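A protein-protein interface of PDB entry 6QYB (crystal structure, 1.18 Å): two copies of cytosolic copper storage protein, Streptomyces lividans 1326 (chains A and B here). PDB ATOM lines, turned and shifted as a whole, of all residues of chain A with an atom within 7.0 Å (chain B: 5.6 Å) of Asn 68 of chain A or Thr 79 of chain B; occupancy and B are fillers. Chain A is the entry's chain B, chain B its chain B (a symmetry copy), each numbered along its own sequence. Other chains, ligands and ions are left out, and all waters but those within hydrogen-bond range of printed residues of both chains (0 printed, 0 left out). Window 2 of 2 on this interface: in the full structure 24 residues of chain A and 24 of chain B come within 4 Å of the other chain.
OD1 of Asp 66 of chain A sits at hydrogen-bond distance from N of Asn 68 of chain A (2.9 Å). The side-chain carboxylate (OD1) of Asp 66 of chain A lies within hydrogen-bond range of the backbone NH (N) of Val 69 of chain A (3.5 Å). The side-chain hydroxyl (OG1) of Thr 70 of chain A is in hydrogen-bond range of the backbone carbonyl oxygen (O) of Asp 66 of chain A. The side-chain amide oxygen of Asn 68 of chain A lies within hydrogen-bond range of the guanidinium group of Arg 71 of chain A. The backbone carbonyl oxygen (O) of Gln 75 of chain B sits at hydrogen-bond distance from the side-chain hydroxyl (OG1) of Thr 79 of chain B, at 2.9 Å.
Asp 66 of chain A touches Ala 83 of chain B. CG2 of Thr 79 of chain B touches O of Asn 68 of chain A (3.7 Å). CG1 of Val 69 of chain A touches CG2 of Val 80 of chain B (3.9 Å). Ala 83 of chain B touches Val 69 of chain A (CB to CG2, 3.8 Å). Ala 76 of chain B touches Ala 72 of chain A (CB to O, 3.7 Å).
Printed residues of chain B within 4 Å of Asp 66 of chain A: Ala 83. Of chain B, only Thr 79 (3.7 Å) comes within 4 Å of Asn 68 of chain A. Printed residues of chain B within 4 Å of Ala 72 of chain A: Ala 76 (3.7 Å). Of the printed residues of chain A, Ala 76 of chain B touches Ala 72 (3.7 Å). Of the printed residues of chain A, Thr 79 of chain B touches Asn 68 (3.7 Å). Printed residues of chain A within 4 Å of Val 80 of chain B: Val 69. Of the printed residues of chain A, Ala 83 of chain B touches Asp 66 and Val 69. The nearest printed residue of chain B that does not touch Asn 68 of chain A is Ala 83 of chain B (6.6 Å). The nearest printed residue of chain A that does not touch Thr 79 of chain B is Val 69 of chain A (4.004 Å). The nearest printed residue of chain B that does not touch Asp 66 of chain A is Thr 79 of chain B (6.2 Å).
Printed residues of chain A that touch a printed residue of chain B: Asp 66, Asn 68, Val 69 and Ala 72. Hydrophobic or aromatic side chains of chain A within 4 Å of the printed part of chain B: Val 69 and Ala 72. Among the printed residues, 5 pairs touch across the chains. Among the printed residues, no Asp or Glu carboxylate lies within 4 Å of a Lys or Arg side-chain nitrogen of the other chain.
No position is printed for both chains. Of the 5 pairs that touch across the chains among the printed residues, none has its exchanged pair printed and touching as well.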
ATOM      1  N   TYR A  65      18.858  19.336  20.973  1.00  0.00           N
ATOM      2  CA  TYR A  65      17.984  20.236  20.171  1.00  0.00           C
ATOM      3  C   TYR A  65      17.727  21.522  20.966  1.00  0.00           C
ATOM      4  O   TYR A  65      17.474  21.444  22.188  1.00  0.00           O
ATOM      5  CB  TYR A  65      16.670  19.532  19.820  1.00  0.00           C
ATOM      6  CG  TYR A  65      15.591  20.423  19.252  1.00  0.00           C
ATOM      7  CD1 TYR A  65      15.664  20.888  17.949  1.00  0.00           C
ATOM      8  CD2 TYR A  65      14.498  20.804  20.017  1.00  0.00           C
ATOM      9  CE1 TYR A  65      14.677  21.702  17.417  1.00  0.00           C
ATOM     10  CE2 TYR A  65      13.515  21.636  19.507  1.00  0.00           C
ATOM     11  CZ  TYR A  65      13.606  22.088  18.201  1.00  0.00           C
ATOM     12  OH  TYR A  65      12.630  22.892  17.689  1.00  0.00           O
ATOM     13  N   ASP A  66      17.779  22.665  20.284  1.00  0.00           N
ATOM     14  CA  ASP A  66      17.477  24.001  20.868  1.00  0.00           C
ATOM     15  C   ASP A  66      16.525  24.735  19.914  1.00  0.00           C
ATOM     16  O   ASP A  66      16.964  25.139  18.844  1.00  0.00           O
ATOM     17  CB  ASP A  66      18.764  24.777  21.174  1.00  0.00           C
ATOM     18  CG  ASP A  66      18.556  26.178  21.735  1.00  0.00           C
ATOM     19  OD1 ASP A  66      17.483  26.762  21.506  1.00  0.00           O
ATOM     20  OD2 ASP A  66      19.477  26.675  22.399  1.00  0.00           O
ATOM     21  N   ALA A  67      15.252  24.884  20.289  1.00  0.00           N
ATOM     22  CA  ALA A  67      14.196  25.476  19.433  1.00  0.00           C
ATOM     23  C   ALA A  67      14.555  26.906  19.013  1.00  0.00           C
ATOM     24  O   ALA A  67      14.163  27.303  17.907  1.00  0.00           O
ATOM     25  CB  ALA A  67      12.868  25.448  20.155  1.00  0.00           C
ATOM     26  N   ASN A  68      15.208  27.679  19.885  1.00  0.00           N
ATOM     27  CA  ASN A  68      15.608  29.078  19.577  1.00  0.00           C
ATOM     28  C   ASN A  68      16.531  29.090  18.362  1.00  0.00           C
ATOM     29  O   ASN A  68      16.322  29.921  17.452  1.00  0.00           O
ATOM     30  CB  ASN A  68      16.318  29.768  20.743  1.00  0.00           C
ATOM     31  CG  ASN A  68      15.435  29.949  21.950  1.00  0.00           C
ATOM     32  OD1 ASN A  68      14.225  30.106  21.806  1.00  0.00           O
ATOM     33  ND2 ASN A  68      16.037  29.943  23.129  1.00  0.00           N
ATOM     34  N   VAL A  69      17.525  28.207  18.367  1.00  0.00           N
ATOM     35  CA  VAL A  69      18.531  28.133  17.272  1.00  0.00           C
ATOM     36  C   VAL A  69      17.793  27.671  16.015  1.00  0.00           C
ATOM     37  O   VAL A  69      17.881  28.330  14.976  1.00  0.00           O
ATOM     38  CB  VAL A  69      19.702  27.207  17.644  1.00  0.00           C
ATOM     39  CG1 VAL A  69      20.572  26.899  16.433  1.00  0.00           C
ATOM     40  CG2 VAL A  69      20.526  27.786  18.780  1.00  0.00           C
ATOM     41  N   THR A  70      17.034  26.588  16.122  1.00  0.00           N
ATOM     42  CA  THR A  70      16.320  25.995  14.965  1.00  0.00           C
ATOM     43  C   THR A  70      15.375  27.042  14.370  1.00  0.00           C
ATOM     44  O   THR A  70      15.373  27.187  13.141  1.00  0.00           O
ATOM     45  CB  THR A  70      15.666  24.669  15.359  1.00  0.00           C
ATOM     46  OG1 THR A  70      16.741  23.822  15.779  1.00  0.00           O
ATOM     47  CG2 THR A  70      14.880  24.047  14.227  1.00  0.00           C
ATOM     48  N   ARG A  71      14.590  27.737  15.204  1.00  0.00           N
ATOM     49  CA  ARG A  71      13.623  28.751  14.714  1.00  0.00           C
ATOM     50  C   ARG A  71      14.368  29.840  13.934  1.00  0.00           C
ATOM     51  O   ARG A  71      13.919  30.212  12.842  1.00  0.00           O
ATOM     52  CB  ARG A  71      12.841  29.382  15.873  1.00  0.00           C
ATOM     53  CG  ARG A  71      11.565  28.654  16.267  1.00  0.00           C
ATOM     54  CD  ARG A  71      10.697  29.535  17.160  1.00  0.00           C
ATOM     55  NE  ARG A  71      11.317  29.755  18.458  1.00  0.00           N
ATOM     56  CZ  ARG A  71      11.061  29.060  19.570  1.00  0.00           C
ATOM     57  NH1 ARG A  71      10.168  28.080  19.576  1.00  0.00           N
ATOM     58  NH2 ARG A  71      11.711  29.357  20.683  1.00  0.00           N
ATOM     59  N   ALA A  72      15.456  30.368  14.491  1.00  0.00           N
ATOM     60  CA  ALA A  72      16.176  31.514  13.892  1.00  0.00           C
ATOM     61  C   ALA A  72      16.813  31.092  12.562  1.00  0.00           C
ATOM     62  O   ALA A  72      16.774  31.866  11.594  1.00  0.00           O
ATOM     63  CB  ALA A  72      17.183  32.080  14.871  1.00  0.00           C
ATOM     64  N   VAL A  73      17.304  29.863  12.480  1.00  0.00           N
ATOM     65  CA  VAL A  73      17.916  29.337  11.228  1.00  0.00           C
ATOM     66  C   VAL A  73      16.794  29.146  10.193  1.00  0.00           C
ATOM     67  O   VAL A  73      16.963  29.574   9.058  1.00  0.00           O
ATOM     68  CB  VAL A  73      18.688  28.037  11.498  1.00  0.00           C
ATOM     69  CG1 VAL A  73      19.074  27.336  10.211  1.00  0.00           C
ATOM     70  CG2 VAL A  73      19.926  28.277  12.347  1.00  0.00           C
ATOM     71  N   LEU B  74      22.222  37.397  10.141  1.00  0.00           N
ATOM     72  CA  LEU B  74      22.943  37.889  11.342  1.00  0.00           C
ATOM     73  C   LEU B  74      22.189  37.489  12.614  1.00  0.00           C
ATOM     74  O   LEU B  74      22.853  37.100  13.594  1.00  0.00           O
ATOM     75  CB  LEU B  74      23.099  39.407  11.272  1.00  0.00           C
ATOM     76  CG  LEU B  74      24.126  39.904  10.260  1.00  0.00           C
ATOM     77  CD1 LEU B  74      23.993  41.407  10.089  1.00  0.00           C
ATOM     78  CD2 LEU B  74      25.546  39.545  10.672  1.00  0.00           C
ATOM     79  N   GLN B  75      20.857  37.548  12.604  1.00  0.00           N
ATOM     80  CA  GLN B  75      20.059  37.136  13.788  1.00  0.00           C
ATOM     81  C   GLN B  75      20.296  35.648  14.068  1.00  0.00           C
ATOM     82  O   GLN B  75      20.491  35.274  15.236  1.00  0.00           O
ATOM     83  CB  GLN B  75      18.562  37.373  13.613  1.00  0.00           C
ATOM     84  CG  GLN B  75      17.800  37.085  14.895  1.00  0.00           C
ATOM     85  CD  GLN B  75      18.350  37.872  16.064  1.00  0.00           C
ATOM     86  OE1 GLN B  75      18.889  37.318  17.025  1.00  0.00           O
ATOM     87  NE2 GLN B  75      18.257  39.184  15.970  1.00  0.00           N
ATOM     88  N   ALA B  76      20.259  34.799  13.042  1.00  0.00           N
ATOM     89  CA  ALA B  76      20.543  33.363  13.229  1.00  0.00           C
ATOM     90  C   ALA B  76      21.945  33.191  13.815  1.00  0.00           C
ATOM     91  O   ALA B  76      22.135  32.407  14.759  1.00  0.00           O
ATOM     92  CB  ALA B  76      20.361  32.614  11.928  1.00  0.00           C
ATOM     93  N   CYS B  77      22.925  33.905  13.290  1.00  0.00           N
ATOM     94  CA  CYS B  77      24.307  33.693  13.761  1.00  0.00           C
ATOM     95  C   CYS B  77      24.464  34.208  15.201  1.00  0.00           C
ATOM     96  O   CYS B  77      25.134  33.536  15.999  1.00  0.00           O
ATOM     97  CB  CYS B  77      25.324  34.307  12.822  1.00  0.00           C
ATOM     98  SG  CYS B  77      26.898  33.444  12.971  1.00  0.00           S
ATOM     99  N   ALA B  78      23.843  35.337  15.549  1.00  0.00           N
ATOM    100  CA  ALA B  78      23.871  35.860  16.937  1.00  0.00           C
ATOM    101  C   ALA B  78      23.261  34.814  17.876  1.00  0.00           C
ATOM    102  O   ALA B  78      23.834  34.515  18.928  1.00  0.00           O
ATOM    103  CB  ALA B  78      23.159  37.193  17.036  1.00  0.00           C
ATOM    104  N   THR B  79      22.147  34.212  17.467  1.00  0.00           N
ATOM    105  CA  THR B  79      21.380  33.249  18.297  1.00  0.00           C
ATOM    106  C   THR B  79      22.223  31.988  18.538  1.00  0.00           C
ATOM    107  O   THR B  79      22.296  31.526  19.694  1.00  0.00           O
ATOM    108  CB  THR B  79      20.007  32.960  17.674  1.00  0.00           C
ATOM    109  OG1 THR B  79      19.313  34.211  17.661  1.00  0.00           O
ATOM    110  CG2 THR B  79      19.232  31.902  18.428  1.00  0.00           C
ATOM    111  N   VAL B  80      22.857  31.433  17.503  1.00  0.00           N
ATOM    112  CA  VAL B  80      23.617  30.168  17.698  1.00  0.00           C
ATOM    113  C   VAL B  80      24.923  30.441  18.455  1.00  0.00           C
ATOM    114  O   VAL B  80      25.282  29.644  19.322  1.00  0.00           O
ATOM    115  CB  VAL B  80      23.851  29.421  16.376  1.00  0.00           C
ATOM    116  CG1 VAL B  80      24.779  30.152  15.427  1.00  0.00           C
ATOM    117  CG2 VAL B  80      24.352  28.015  16.646  1.00  0.00           C
ATOM    118  N   CYS B  81      25.583  31.565  18.200  1.00  0.00           N
ATOM    119  CA  CYS B  81      26.805  31.944  18.950  1.00  0.00           C
ATOM    120  C   CYS B  81      26.463  32.093  20.438  1.00  0.00           C
ATOM    121  O   CYS B  81      27.254  31.634  21.278  1.00  0.00           O
ATOM    122  CB  CYS B  81      27.429  33.241  18.451  1.00  0.00           C
ATOM    123  SG  CYS B  81      28.427  33.019  16.952  1.00  0.00           S
ATOM    124  N   ALA B  82      25.317  32.697  20.755  1.00  0.00           N
ATOM    125  CA  ALA B  82      24.868  32.874  22.154  1.00  0.00           C
ATOM    126  C   ALA B  82      24.685  31.488  22.782  1.00  0.00           C
ATOM    127  O   ALA B  82      25.207  31.238  23.879  1.00  0.00           O
ATOM    128  CB  ALA B  82      23.610  33.703  22.214  1.00  0.00           C
ATOM    129  N   ALA B  83      23.993  30.586  22.091  1.00  0.00           N
ATOM    130  CA  ALA B  83      23.704  29.236  22.623  1.00  0.00           C
ATOM    131  C   ALA B  83      25.016  28.455  22.775  1.00  0.00           C
ATOM    132  O   ALA B  83      25.208  27.748  23.782  1.00  0.00           O
ATOM    133  CB  ALA B  83      22.738  28.521  21.718  1.00  0.00           C
ATOM    134  N   CYS B  84      25.890  28.525  21.772  1.00  0.00           N
ATOM    135  CA  CYS B  84      27.123  27.718  21.781  1.00  0.00           C
ATOM    136  C   CYS B  84      28.128  28.285  22.787  1.00  0.00           C
ATOM    137  O   CYS B  84      28.848  27.497  23.420  1.00  0.00           O
ATOM    138  CB  CYS B  84      27.734  27.638  20.395  1.00  0.00           C
ATOM    139  SG  CYS B  84      28.775  26.172  20.266  1.00  0.00           S
